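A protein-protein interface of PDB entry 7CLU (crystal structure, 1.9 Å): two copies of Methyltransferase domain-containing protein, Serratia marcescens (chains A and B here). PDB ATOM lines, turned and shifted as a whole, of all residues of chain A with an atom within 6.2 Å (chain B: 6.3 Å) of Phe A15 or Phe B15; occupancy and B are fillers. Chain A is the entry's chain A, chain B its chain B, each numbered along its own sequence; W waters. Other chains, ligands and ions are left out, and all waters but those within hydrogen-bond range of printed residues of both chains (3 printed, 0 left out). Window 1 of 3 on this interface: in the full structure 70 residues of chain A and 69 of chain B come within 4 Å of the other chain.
The side-chain amino group of Lys B19 lies within hydrogen-bond range of the backbone carbonyl oxygen of Gly A108. O of Tyr A104 sits at hydrogen-bond distance from OH of Tyr B104, 2.8 Å away.
The backbone carbonyl oxygen (O) of Ile B99 is in hydrogen-bond range of the backbone NH (N) of Tyr B104 (2.8 Å). O of Ile A99 sits at hydrogen-bond distance from N of Tyr A104, at 2.9 Å. O of Met A13 lies close to OE1 of Gln A17, 3.5 Å away. The side-chain amide oxygen (OD1) of Asn B294 sits at hydrogen-bond distance from the indole nitrogen (NE1) of Trp B107. The backbone carbonyl oxygen (O) of Gly B14 lies close to the side-chain amide oxygen (OE1) of Gln B17. The backbone carbonyl oxygen of Met B13 sits close to the side-chain amide oxygen of Gln B17 (3.5 Å).
Among the printed residues, pairs that only touch across the chains: Gln A11 with Gln B17 (3.7 Å), Gln A11 with Ala B18 (3.1 Å), Met A12 with Ala B18 (3.4 Å), Met A12 with Ile B99 (3.5 Å), Met A13 with Ile B99 (3.7 Å), Phe A15 with Phe B15 (3.9 Å), Phe A15 with Ile B99 (3.6 Å), Phe A15 with Leu B103 (3.8 Å), Phe A15 with Tyr B104 (3.8 Å), Phe A15 with Trp B107 (3.9 Å), Phe A16 with Trp B107 (3.3 Å), Phe A16 with Asn B294 (3.7 Å), Gln A17 with Gln B11 (3.7 Å), Ala A18 with Gln B11 (3.3 Å), Ala A18 with Met B12 (3.4 Å), Lys A19 with Trp B107 (3.4 Å), Ile A99 with Met B12 (3.5 Å), Ile A99 with Phe B15 (3.6 Å), Leu A103 with Met B13 (3.9 Å), Leu A103 with Phe B15 (3.7 Å), Tyr A104 with Phe B15 (3.6 Å), Tyr A104 with Trp B107 (3.7 Å), Trp A107 with Phe B15 (3.7 Å), Trp A107 with Phe B16 (3.2 Å), Trp A107 with Lys B19 (3.2 Å), Trp A107 with Tyr B104 (3.6 Å), Gly A108 with Tyr B104 (3.5 Å) and Asn A294 with Phe B16 (3.5 Å).
Of chain B, only Phe B15 (3.9 Å), Ile B99 (3.6 Å), Leu B103 (3.8 Å), Tyr B104 (3.8 Å) and Trp B107 (3.9 Å) come within 4 Å of Phe A15. Printed residues of chain B within 4 Å of Gly A108: Lys B19 and Tyr B104. Of the printed residues of chain B, Asn A294 touches Phe B16. Printed residues of chain A within 4 Å of Ala B18: Gln A11 (3.1 Å) and Met A12 (3.4 Å). Printed residues of chain A within 4 Å of Lys B19: Trp A107 and Gly A108. Of the printed residues of chain A, Asn B294 touches Phe A16 (3.7 Å). The nearest residue of chain B that does not touch Phe A15 is Ala B18 (4.1 Å). The nearest residue of chain A that does not touch Phe B15 is Ala A18 (4.1 Å).
Of the 17 printed residues of chain B, 13 touch a printed residue of chain A. Hydrophobic or aromatic side chains of chain B within 4 Å of the printed part of chain A: Met B12, Met B13, Phe B15, Phe B16, Ala B18, Ile B99, Leu B103, Tyr B104 and Trp B107. Hydrophobic or aromatic side chains of chain A that line the printed part of chain B: Met A12, Met A13, Phe A15, Phe A16, Ala A18, Ile A99, Leu A103, Tyr A104 and Trp A107. Along chain A the printed residues that touch a printed residue of chain B span positions 11 to 294. Among the printed residues, 30 pairs touch across the chains. Among the printed residues, no Asp or Glu carboxylate lies within 4 Å of a Lys or Arg side-chain nitrogen of the other chain.
Phe A15 touches its own counterpart, Phe B15. Phe A15 touches Leu B103, and with the chains exchanged Leu A103 touches Phe B15. Phe A15 touches Trp B107, and with the chains exchanged Trp A107 touches Phe B15. Phe A16 touches Trp B107, and with the chains exchanged Trp A107 touches Phe B16. Positions printed for both chains: 10, 11, 12, 13, 14, 15, 16, 17, 18, 19, 20, 99, 103, 104, 105, 107 and 294. Of the 30 pairs that touch across the chains among the printed residues, 26 have their exchanged pair printed and touching as well.
Water W1 lies within hydrogen-bond range of the backbone carbonyl oxygen (O) of Gln B11 and the backbone carbonyl oxygen (O) of Gly A14. Water W2 lies within hydrogen-bond range of O of Gln A11 (2.7 Å) and O of Gly B14 (2.9 Å). Water W3 lies within hydrogen-bond range of O of Gly A108 and NZ of Lys B19.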
ATOM      1  N   ASN A  10       5.674 -10.285  -2.406  1.00  0.00           N
ATOM      2  CA  ASN A  10       4.959  -9.015  -2.514  1.00  0.00           C
ATOM      3  C   ASN A  10       4.633  -8.686  -3.966  1.00  0.00           C
ATOM      4  O   ASN A  10       3.506  -8.289  -4.295  1.00  0.00           O
ATOM      5  CB  ASN A  10       5.795  -7.890  -1.892  1.00  0.00           C
ATOM      6  CG  ASN A  10       5.762  -7.906  -0.368  1.00  0.00           C
ATOM      7  OD1 ASN A  10       4.838  -8.449   0.232  1.00  0.00           O
ATOM      8  ND2 ASN A  10       6.785  -7.340   0.256  1.00  0.00           N
ATOM      9  N   GLN A  11       5.607  -8.852  -4.859  1.00  0.00           N
ATOM     10  CA  GLN A  11       5.337  -8.478  -6.244  1.00  0.00           C
ATOM     11  C   GLN A  11       4.470  -9.500  -6.966  1.00  0.00           C
ATOM     12  O   GLN A  11       3.618  -9.116  -7.776  1.00  0.00           O
ATOM     13  CB  GLN A  11       6.643  -8.246  -6.986  1.00  0.00           C
ATOM     14  CG  GLN A  11       7.450  -7.143  -6.381  1.00  0.00           C
ATOM     15  CD  GLN A  11       8.441  -6.565  -7.354  1.00  0.00           C
ATOM     16  OE1 GLN A  11       9.610  -6.964  -7.379  1.00  0.00           O
ATOM     17  NE2 GLN A  11       7.981  -5.619  -8.174  1.00  0.00           N
ATOM     18  N   MET A  12       4.635 -10.798  -6.673  1.00  0.00           N
ATOM     19  CA  MET A  12       3.753 -11.794  -7.268  1.00  0.00           C
ATOM     20  C   MET A  12       2.290 -11.561  -6.887  1.00  0.00           C
ATOM     21  O   MET A  12       1.393 -11.951  -7.641  1.00  0.00           O
ATOM     22  CB  MET A  12       4.188 -13.209  -6.863  1.00  0.00           C
ATOM     23  CG  MET A  12       5.519 -13.658  -7.468  1.00  0.00           C
ATOM     24  SD  MET A  12       6.254 -15.061  -6.575  1.00  0.00           S
ATOM     25  CE  MET A  12       5.009 -16.308  -6.878  1.00  0.00           C
ATOM     26  N   MET A  13       2.031 -10.919  -5.743  1.00  0.00           N
ATOM     27  CA  MET A  13       0.672 -10.611  -5.298  1.00  0.00           C
ATOM     28  C   MET A  13       0.220  -9.211  -5.690  1.00  0.00           C
ATOM     29  O   MET A  13      -0.889  -8.804  -5.322  1.00  0.00           O
ATOM     30  CB  MET A  13       0.561 -10.736  -3.774  1.00  0.00           C
ATOM     31  CG  MET A  13       1.171 -11.999  -3.224  1.00  0.00           C
ATOM     32  SD  MET A  13       0.325 -13.419  -3.895  1.00  0.00           S
ATOM     33  CE  MET A  13      -1.026 -13.472  -2.722  1.00  0.00           C
ATOM     34  N   GLY A  14       1.048  -8.469  -6.421  1.00  0.00           N
ATOM     35  CA  GLY A  14       0.727  -7.101  -6.782  1.00  0.00           C
ATOM     36  C   GLY A  14      -0.456  -6.950  -7.715  1.00  0.00           C
ATOM     37  O   GLY A  14      -0.936  -5.819  -7.890  1.00  0.00           O
ATOM     38  N   PHE A  15      -0.929  -8.048  -8.327  1.00  0.00           N
ATOM     39  CA  PHE A  15      -2.204  -7.980  -9.037  1.00  0.00           C
ATOM     40  C   PHE A  15      -3.362  -7.690  -8.084  1.00  0.00           C
ATOM     41  O   PHE A  15      -4.387  -7.153  -8.533  1.00  0.00           O
ATOM     42  CB  PHE A  15      -2.458  -9.271  -9.866  1.00  0.00           C
ATOM     43  CG  PHE A  15      -2.646 -10.522  -9.027  1.00  0.00           C
ATOM     44  CD1 PHE A  15      -1.553 -11.219  -8.541  1.00  0.00           C
ATOM     45  CD2 PHE A  15      -3.920 -11.001  -8.745  1.00  0.00           C
ATOM     46  CE1 PHE A  15      -1.726 -12.360  -7.754  1.00  0.00           C
ATOM     47  CE2 PHE A  15      -4.096 -12.147  -7.960  1.00  0.00           C
ATOM     48  CZ  PHE A  15      -2.989 -12.813  -7.464  1.00  0.00           C
ATOM     49  N   PHE A  16      -3.199  -7.955  -6.777  1.00  0.00           N
ATOM     50  CA  PHE A  16      -4.197  -7.530  -5.783  1.00  0.00           C
ATOM     51  C   PHE A  16      -4.450  -6.025  -5.850  1.00  0.00           C
ATOM     52  O   PHE A  16      -5.594  -5.576  -5.986  1.00  0.00           O
ATOM     53  CB  PHE A  16      -3.749  -7.869  -4.359  1.00  0.00           C
ATOM     54  CG  PHE A  16      -3.882  -9.308  -3.983  1.00  0.00           C
ATOM     55  CD1 PHE A  16      -4.235 -10.273  -4.915  1.00  0.00           C
ATOM     56  CD2 PHE A  16      -3.640  -9.700  -2.665  1.00  0.00           C
ATOM     57  CE1 PHE A  16      -4.339 -11.608  -4.547  1.00  0.00           C
ATOM     58  CE2 PHE A  16      -3.759 -11.035  -2.284  1.00  0.00           C
ATOM     59  CZ  PHE A  16      -4.106 -11.993  -3.234  1.00  0.00           C
ATOM     60  N   GLN A  17      -3.394  -5.229  -5.661  1.00  0.00           N
ATOM     61  CA  GLN A  17      -3.563  -3.784  -5.650  1.00  0.00           C
ATOM     62  C   GLN A  17      -4.075  -3.296  -6.993  1.00  0.00           C
ATOM     63  O   GLN A  17      -4.887  -2.367  -7.053  1.00  0.00           O
ATOM     64  CB  GLN A  17      -2.245  -3.088  -5.297  1.00  0.00           C
ATOM     65  CG  GLN A  17      -1.812  -3.240  -3.827  1.00  0.00           C
ATOM     66  CD  GLN A  17      -0.901  -4.458  -3.601  1.00  0.00           C
ATOM     67  OE1 GLN A  17      -1.074  -5.518  -4.221  1.00  0.00           O
ATOM     68  NE2 GLN A  17       0.078  -4.300  -2.708  1.00  0.00           N
ATOM     69  N   ALA A  18      -3.610  -3.917  -8.083  1.00  0.00           N
ATOM     70  CA  ALA A  18      -4.022  -3.476  -9.413  1.00  0.00           C
ATOM     71  C   ALA A  18      -5.530  -3.586  -9.577  1.00  0.00           C
ATOM     72  O   ALA A  18      -6.191  -2.630  -9.983  1.00  0.00           O
ATOM     73  CB  ALA A  18      -3.298  -4.298 -10.492  1.00  0.00           C
ATOM     74  N   LYS A  19      -6.092  -4.755  -9.249  1.00  0.00           N
ATOM     75  CA  LYS A  19      -7.522  -4.986  -9.442  1.00  0.00           C
ATOM     76  C   LYS A  19      -8.374  -4.284  -8.392  1.00  0.00           C
ATOM     77  O   LYS A  19      -9.532  -3.945  -8.678  1.00  0.00           O
ATOM     78  CB  LYS A  19      -7.827  -6.486  -9.446  1.00  0.00           C
ATOM     79  CG  LYS A  19      -7.610  -7.161 -10.799  1.00  0.00           C
ATOM     80  CD  LYS A  19      -8.667  -6.696 -11.800  1.00  0.00           C
ATOM     81  CE  LYS A  19      -8.600  -7.481 -13.089  1.00  0.00           C
ATOM     82  NZ  LYS A  19      -9.831  -7.293 -13.916  1.00  0.00           N
ATOM     83  N   ALA A  20      -7.847  -4.039  -7.183  1.00  0.00           N
ATOM     84  CA  ALA A  20      -8.589  -3.177  -6.263  1.00  0.00           C
ATOM     85  C   ALA A  20      -8.789  -1.792  -6.875  1.00  0.00           C
ATOM     86  O   ALA A  20      -9.885  -1.228  -6.818  1.00  0.00           O
ATOM     87  CB  ALA A  20      -7.883  -3.068  -4.905  1.00  0.00           C
ATOM     88  N   ILE A  99      -7.286  -2.217 -18.934  1.00  0.00           N
ATOM     89  CA  ILE A  99      -6.734  -3.308 -18.135  1.00  0.00           C
ATOM     90  C   ILE A  99      -7.771  -4.412 -17.941  1.00  0.00           C
ATOM     91  O   ILE A  99      -7.507  -5.587 -18.217  1.00  0.00           O
ATOM     92  CB  ILE A  99      -6.212  -2.766 -16.785  1.00  0.00           C
ATOM     93  CG1 ILE A  99      -4.881  -2.035 -16.995  1.00  0.00           C
ATOM     94  CG2 ILE A  99      -6.038  -3.909 -15.779  1.00  0.00           C
ATOM     95  CD1 ILE A  99      -4.555  -0.958 -15.957  1.00  0.00           C
ATOM     96  N   LEU A 103      -5.735  -5.973 -21.226  1.00  0.00           N
ATOM     97  CA  LEU A 103      -4.366  -6.302 -20.810  1.00  0.00           C
ATOM     98  C   LEU A 103      -4.319  -7.350 -19.692  1.00  0.00           C
ATOM     99  O   LEU A 103      -3.450  -8.229 -19.698  1.00  0.00           O
ATOM    100  CB  LEU A 103      -3.633  -5.040 -20.378  1.00  0.00           C
ATOM    101  CG  LEU A 103      -3.390  -4.011 -21.486  1.00  0.00           C
ATOM    102  CD1 LEU A 103      -2.395  -2.953 -21.014  1.00  0.00           C
ATOM    103  CD2 LEU A 103      -2.886  -4.713 -22.715  1.00  0.00           C
ATOM    104  N   TYR A 104      -5.174  -7.229 -18.678  1.00  0.00           N
ATOM    105  CA  TYR A 104      -5.132  -8.211 -17.596  1.00  0.00           C
ATOM    106  C   TYR A 104      -5.404  -9.616 -18.115  1.00  0.00           C
ATOM    107  O   TYR A 104      -4.618 -10.527 -17.799  1.00  0.00           O
ATOM    108  CB  TYR A 104      -6.108  -7.792 -16.496  1.00  0.00           C
ATOM    109  CG  TYR A 104      -6.052  -8.615 -15.235  1.00  0.00           C
ATOM    110  CD1 TYR A 104      -6.790  -9.801 -15.112  1.00  0.00           C
ATOM    111  CD2 TYR A 104      -5.279  -8.207 -14.160  1.00  0.00           C
ATOM    112  CE1 TYR A 104      -6.757 -10.550 -13.937  1.00  0.00           C
ATOM    113  CE2 TYR A 104      -5.243  -8.938 -12.978  1.00  0.00           C
ATOM    114  CZ  TYR A 104      -5.976 -10.107 -12.869  1.00  0.00           C
ATOM    115  OH  TYR A 104      -5.920 -10.824 -11.680  1.00  0.00           O
ATOM    116  N   PRO A 105      -6.442  -9.867 -18.926  1.00  0.00           N
ATOM    117  CA  PRO A 105      -6.620 -11.239 -19.436  1.00  0.00           C
ATOM    118  C   PRO A 105      -5.422 -11.741 -20.229  1.00  0.00           C
ATOM    119  O   PRO A 105      -5.022 -12.897 -20.064  1.00  0.00           O
ATOM    120  CB  PRO A 105      -7.883 -11.136 -20.305  1.00  0.00           C
ATOM    121  CG  PRO A 105      -8.584  -9.938 -19.828  1.00  0.00           C
ATOM    122  CD  PRO A 105      -7.537  -8.981 -19.363  1.00  0.00           C
ATOM    123  N   TRP A 107      -2.164 -10.836 -20.052  1.00  0.00           N
ATOM    124  CA  TRP A 107      -1.009 -11.154 -19.223  1.00  0.00           C
ATOM    125  C   TRP A 107      -1.214 -12.418 -18.409  1.00  0.00           C
ATOM    126  O   TRP A 107      -0.231 -13.000 -17.937  1.00  0.00           O
ATOM    127  CB  TRP A 107      -0.667 -10.001 -18.279  1.00  0.00           C
ATOM    128  CG  TRP A 107       0.143  -8.917 -18.928  1.00  0.00           C
ATOM    129  CD1 TRP A 107      -0.307  -7.976 -19.810  1.00  0.00           C
ATOM    130  CD2 TRP A 107       1.533  -8.634 -18.707  1.00  0.00           C
ATOM    131  NE1 TRP A 107       0.724  -7.131 -20.161  1.00  0.00           N
ATOM    132  CE2 TRP A 107       1.862  -7.517 -19.501  1.00  0.00           C
ATOM    133  CE3 TRP A 107       2.537  -9.234 -17.929  1.00  0.00           C
ATOM    134  CZ2 TRP A 107       3.156  -6.966 -19.526  1.00  0.00           C
ATOM    135  CZ3 TRP A 107       3.820  -8.699 -17.965  1.00  0.00           C
ATOM    136  CH2 TRP A 107       4.114  -7.564 -18.749  1.00  0.00           C
ATOM    137  N   GLY A 108      -2.458 -12.847 -18.222  1.00  0.00           N
ATOM    138  CA  GLY A 108      -2.685 -14.141 -17.607  1.00  0.00           C
ATOM    139  C   GLY A 108      -1.975 -15.252 -18.352  1.00  0.00           C
ATOM    140  O   GLY A 108      -1.548 -16.234 -17.749  1.00  0.00           O
ATOM    141  N   ASN A 294       4.277  -6.224 -22.590  1.00  0.00           N
ATOM    142  CA  ASN A 294       2.908  -5.869 -22.950  1.00  0.00           C
ATOM    143  C   ASN A 294       2.725  -5.884 -24.465  1.00  0.00           C
ATOM    144  O   ASN A 294       1.680  -6.311 -24.963  1.00  0.00           O
ATOM    145  CB  ASN A 294       2.536  -4.504 -22.371  1.00  0.00           C
ATOM    146  CG  ASN A 294       1.053  -4.182 -22.530  1.00  0.00           C
ATOM    147  OD1 ASN A 294       0.216  -4.794 -21.887  1.00  0.00           O
ATOM    148  ND2 ASN A 294       0.730  -3.201 -23.374  1.00  0.00           N
ATOM    149  N   ASN B  10       1.190   3.149 -11.882  1.00  0.00           N
ATOM    150  CA  ASN B  10       2.149   2.081 -11.610  1.00  0.00           C
ATOM    151  C   ASN B  10       1.506   0.929 -10.851  1.00  0.00           C
ATOM    152  O   ASN B  10       1.802  -0.243 -11.115  1.00  0.00           O
ATOM    153  CB  ASN B  10       3.340   2.639 -10.830  1.00  0.00           C
ATOM    154  CG  ASN B  10       4.106   3.678 -11.626  1.00  0.00           C
ATOM    155  OD1 ASN B  10       4.109   3.648 -12.857  1.00  0.00           O
ATOM    156  ND2 ASN B  10       4.727   4.621 -10.930  1.00  0.00           N
ATOM    157  N   GLN B  11       0.610   1.235  -9.922  1.00  0.00           N
ATOM    158  CA  GLN B  11      -0.017   0.159  -9.173  1.00  0.00           C
ATOM    159  C   GLN B  11      -1.088  -0.548  -9.999  1.00  0.00           C
ATOM    160  O   GLN B  11      -1.257  -1.768  -9.885  1.00  0.00           O
ATOM    161  CB  GLN B  11      -0.589   0.708  -7.868  1.00  0.00           C
ATOM    162  CG  GLN B  11       0.401   0.588  -6.724  1.00  0.00           C
ATOM    163  CD  GLN B  11      -0.216   0.899  -5.386  1.00  0.00           C
ATOM    164  OE1 GLN B  11      -0.785   1.971  -5.194  1.00  0.00           O
ATOM    165  NE2 GLN B  11      -0.102  -0.032  -4.451  1.00  0.00           N
ATOM    166  N   MET B  12      -1.827   0.201 -10.819  1.00  0.00           N
ATOM    167  CA  MET B  12      -2.816  -0.396 -11.707  1.00  0.00           C
ATOM    168  C   MET B  12      -2.178  -1.376 -12.682  1.00  0.00           C
ATOM    169  O   MET B  12      -2.857  -2.288 -13.170  1.00  0.00           O
ATOM    170  CB  MET B  12      -3.563   0.696 -12.487  1.00  0.00           C
ATOM    171  CG  MET B  12      -4.615   1.480 -11.680  1.00  0.00           C
ATOM    172  SD  MET B  12      -5.045   3.010 -12.548  1.00  0.00           S
ATOM    173  CE  MET B  12      -5.971   2.303 -13.931  1.00  0.00           C
ATOM    174  N   MET B  13      -0.877  -1.211 -12.932  1.00  0.00           N
ATOM    175  CA  MET B  13      -0.146  -2.094 -13.879  1.00  0.00           C
ATOM    176  C   MET B  13       0.768  -3.066 -13.119  1.00  0.00           C
ATOM    177  O   MET B  13       1.581  -3.730 -13.780  1.00  0.00           O
ATOM    178  CB  MET B  13       0.689  -1.268 -14.860  1.00  0.00           C
ATOM    179  CG  MET B  13      -0.070  -0.105 -15.460  1.00  0.00           C
ATOM    180  SD  MET B  13       0.218   0.095 -17.230  1.00  0.00           S
ATOM    181  CE  MET B  13      -0.796  -1.236 -17.870  1.00  0.00           C
ATOM    182  N   GLY B  14       0.640  -3.141 -11.791  1.00  0.00           N
ATOM    183  CA  GLY B  14       1.456  -4.052 -11.000  1.00  0.00           C
ATOM    184  C   GLY B  14       1.299  -5.515 -11.370  1.00  0.00           C
ATOM    185  O   GLY B  14       2.160  -6.329 -11.019  1.00  0.00           O
ATOM    186  N   PHE B  15       0.205  -5.879 -12.044  1.00  0.00           N
ATOM    187  CA  PHE B  15       0.083  -7.237 -12.556  1.00  0.00           C
ATOM    188  C   PHE B  15       1.150  -7.542 -13.599  1.00  0.00           C
ATOM    189  O   PHE B  15       1.442  -8.721 -13.832  1.00  0.00           O
ATOM    190  CB  PHE B  15      -1.335  -7.498 -13.110  1.00  0.00           C
ATOM    191  CG  PHE B  15      -1.694  -6.714 -14.360  1.00  0.00           C
ATOM    192  CD1 PHE B  15      -2.134  -5.394 -14.273  1.00  0.00           C
ATOM    193  CD2 PHE B  15      -1.659  -7.316 -15.607  1.00  0.00           C
ATOM    194  CE1 PHE B  15      -2.505  -4.688 -15.416  1.00  0.00           C
ATOM    195  CE2 PHE B  15      -2.006  -6.618 -16.757  1.00  0.00           C
ATOM    196  CZ  PHE B  15      -2.433  -5.302 -16.662  1.00  0.00           C
ATOM    197  N   PHE B  16       1.745  -6.507 -14.218  1.00  0.00           N
ATOM    198  CA  PHE B  16       2.925  -6.698 -15.068  1.00  0.00           C
ATOM    199  C   PHE B  16       4.031  -7.430 -14.320  1.00  0.00           C
ATOM    200  O   PHE B  16       4.518  -8.483 -14.760  1.00  0.00           O
ATOM    201  CB  PHE B  16       3.489  -5.355 -15.545  1.00  0.00           C
ATOM    202  CG  PHE B  16       2.765  -4.745 -16.694  1.00  0.00           C
ATOM    203  CD1 PHE B  16       1.538  -5.225 -17.112  1.00  0.00           C
ATOM    204  CD2 PHE B  16       3.322  -3.671 -17.362  1.00  0.00           C
ATOM    205  CE1 PHE B  16       0.881  -4.638 -18.184  1.00  0.00           C
ATOM    206  CE2 PHE B  16       2.662  -3.070 -18.429  1.00  0.00           C
ATOM    207  CZ  PHE B  16       1.446  -3.556 -18.840  1.00  0.00           C
ATOM    208  N   GLN B  17       4.484  -6.834 -13.214  1.00  0.00           N
ATOM    209  CA  GLN B  17       5.553  -7.426 -12.417  1.00  0.00           C
ATOM    210  C   GLN B  17       5.158  -8.796 -11.898  1.00  0.00           C
ATOM    211  O   GLN B  17       5.989  -9.711 -11.862  1.00  0.00           O
ATOM    212  CB  GLN B  17       5.891  -6.514 -11.234  1.00  0.00           C
ATOM    213  CG  GLN B  17       6.706  -5.292 -11.591  1.00  0.00           C
ATOM    214  CD  GLN B  17       5.865  -4.117 -12.042  1.00  0.00           C
ATOM    215  OE1 GLN B  17       4.645  -4.216 -12.254  1.00  0.00           O
ATOM    216  NE2 GLN B  17       6.519  -2.985 -12.180  1.00  0.00           N
ATOM    217  N   ALA B  18       3.902  -8.941 -11.458  1.00  0.00           N
ATOM    218  CA  ALA B  18       3.456 -10.190 -10.854  1.00  0.00           C
ATOM    219  C   ALA B  18       3.544 -11.334 -11.860  1.00  0.00           C
ATOM    220  O   ALA B  18       4.106 -12.397 -11.565  1.00  0.00           O
ATOM    221  CB  ALA B  18       2.029 -10.034 -10.325  1.00  0.00           C
ATOM    222  N   LYS B  19       3.045 -11.111 -13.078  1.00  0.00           N
ATOM    223  CA  LYS B  19       3.089 -12.169 -14.081  1.00  0.00           C
ATOM    224  C   LYS B  19       4.494 -12.405 -14.620  1.00  0.00           C
ATOM    225  O   LYS B  19       4.796 -13.528 -15.053  1.00  0.00           O
ATOM    226  CB  LYS B  19       2.120 -11.864 -15.227  1.00  0.00           C
ATOM    227  CG  LYS B  19       0.694 -12.349 -14.956  1.00  0.00           C
ATOM    228  CD  LYS B  19       0.619 -13.893 -14.901  1.00  0.00           C
ATOM    229  CE  LYS B  19      -0.743 -14.411 -14.422  1.00  0.00           C
ATOM    230  NZ  LYS B  19      -1.008 -15.833 -14.900  1.00  0.00           N
ATOM    231  N   ALA B  20       5.368 -11.384 -14.624  1.00  0.00           N
ATOM    232  CA  ALA B  20       6.749 -11.638 -15.036  1.00  0.00           C
ATOM    233  C   ALA B  20       7.395 -12.664 -14.113  1.00  0.00           C
ATOM    234  O   ALA B  20       8.096 -13.584 -14.569  1.00  0.00           O
ATOM    235  CB  ALA B  20       7.561 -10.341 -15.055  1.00  0.00           C
ATOM    236  N   ILE B  99      -1.192 -18.754  -7.966  1.00  0.00           N
ATOM    237  CA  ILE B  99      -1.601 -17.486  -8.583  1.00  0.00           C
ATOM    238  C   ILE B  99      -2.096 -17.723 -10.003  1.00  0.00           C
ATOM    239  O   ILE B  99      -3.173 -17.258 -10.390  1.00  0.00           O
ATOM    240  CB  ILE B  99      -0.451 -16.458  -8.557  1.00  0.00           C
ATOM    241  CG1 ILE B  99      -0.246 -15.888  -7.144  1.00  0.00           C
ATOM    242  CG2 ILE B  99      -0.742 -15.306  -9.534  1.00  0.00           C
ATOM    243  CD1 ILE B  99       1.174 -15.352  -6.906  1.00  0.00           C
ATOM    244  N   LEU B 103      -5.785 -17.710  -8.261  1.00  0.00           N
ATOM    245  CA  LEU B 103      -6.031 -16.360  -7.747  1.00  0.00           C
ATOM    246  C   LEU B 103      -6.130 -15.334  -8.867  1.00  0.00           C
ATOM    247  O   LEU B 103      -7.059 -14.510  -8.889  1.00  0.00           O
ATOM    248  CB  LEU B 103      -4.935 -15.964  -6.758  1.00  0.00           C
ATOM    249  CG  LEU B 103      -4.836 -16.856  -5.513  1.00  0.00           C
ATOM    250  CD1 LEU B 103      -3.947 -16.242  -4.452  1.00  0.00           C
ATOM    251  CD2 LEU B 103      -6.213 -17.138  -4.956  1.00  0.00           C
ATOM    252  N   TYR B 104      -5.172 -15.349  -9.798  1.00  0.00           N
ATOM    253  CA  TYR B 104      -5.186 -14.347 -10.862  1.00  0.00           C
ATOM    254  C   TYR B 104      -6.471 -14.397 -11.669  1.00  0.00           C
ATOM    255  O   TYR B 104      -7.073 -13.333 -11.888  1.00  0.00           O
ATOM    256  CB  TYR B 104      -3.950 -14.515 -11.746  1.00  0.00           C
ATOM    257  CG  TYR B 104      -3.734 -13.423 -12.755  1.00  0.00           C
ATOM    258  CD1 TYR B 104      -4.372 -13.452 -13.990  1.00  0.00           C
ATOM    259  CD2 TYR B 104      -2.848 -12.379 -12.491  1.00  0.00           C
ATOM    260  CE1 TYR B 104      -4.156 -12.473 -14.924  1.00  0.00           C
ATOM    261  CE2 TYR B 104      -2.602 -11.410 -13.428  1.00  0.00           C
ATOM    262  CZ  TYR B 104      -3.268 -11.440 -14.633  1.00  0.00           C
ATOM    263  OH  TYR B 104      -3.032 -10.440 -15.554  1.00  0.00           O
ATOM    264  N   PRO B 105      -6.963 -15.563 -12.123  1.00  0.00           N
ATOM    265  CA  PRO B 105      -8.280 -15.553 -12.776  1.00  0.00           C
ATOM    266  C   PRO B 105      -9.391 -15.109 -11.841  1.00  0.00           C
ATOM    267  O   PRO B 105     -10.275 -14.347 -12.245  1.00  0.00           O
ATOM    268  CB  PRO B 105      -8.467 -17.007 -13.232  1.00  0.00           C
ATOM    269  CG  PRO B 105      -7.120 -17.613 -13.194  1.00  0.00           C
ATOM    270  CD  PRO B 105      -6.360 -16.908 -12.127  1.00  0.00           C
ATOM    271  N   TRP B 107      -9.292 -13.021  -9.324  1.00  0.00           N
ATOM    272  CA  TRP B 107      -9.292 -11.573  -9.149  1.00  0.00           C
ATOM    273  C   TRP B 107      -9.651 -10.818 -10.416  1.00  0.00           C
ATOM    274  O   TRP B 107      -9.962  -9.622 -10.332  1.00  0.00           O
ATOM    275  CB  TRP B 107      -7.943 -11.115  -8.649  1.00  0.00           C
ATOM    276  CG  TRP B 107      -7.808 -11.252  -7.178  1.00  0.00           C
ATOM    277  CD1 TRP B 107      -7.700 -12.409  -6.465  1.00  0.00           C
ATOM    278  CD2 TRP B 107      -7.733 -10.185  -6.235  1.00  0.00           C
ATOM    279  NE1 TRP B 107      -7.561 -12.120  -5.117  1.00  0.00           N
ATOM    280  CE2 TRP B 107      -7.580 -10.761  -4.954  1.00  0.00           C
ATOM    281  CE3 TRP B 107      -7.784  -8.794  -6.345  1.00  0.00           C
ATOM    282  CZ2 TRP B 107      -7.465  -9.984  -3.792  1.00  0.00           C
ATOM    283  CZ3 TRP B 107      -7.671  -8.023  -5.175  1.00  0.00           C
ATOM    284  CH2 TRP B 107      -7.510  -8.620  -3.936  1.00  0.00           C
ATOM    285  N   ASN B 294      -9.297 -11.062  -1.244  1.00  0.00           N
ATOM    286  CA  ASN B 294      -8.979 -12.395  -1.743  1.00  0.00           C
ATOM    287  C   ASN B 294      -9.964 -13.428  -1.206  1.00  0.00           C
ATOM    288  O   ASN B 294     -10.378 -14.336  -1.936  1.00  0.00           O
ATOM    289  CB  ASN B 294      -7.543 -12.798  -1.399  1.00  0.00           C
ATOM    290  CG  ASN B 294      -7.130 -14.113  -2.076  1.00  0.00           C
ATOM    291  OD1 ASN B 294      -7.083 -14.196  -3.296  1.00  0.00           O
ATOM    292  ND2 ASN B 294      -6.853 -15.151  -1.276  1.00  0.00           N
HETATM  293  O   HOH W   1      -0.014  -3.261  -8.132  1.00  0.00           O
HETATM  294  O   HOH W   2       3.615  -6.557  -8.521  1.00  0.00           O
HETATM  295  O   HOH W   3      -1.868 -18.744 -16.447  1.00  0.00           O
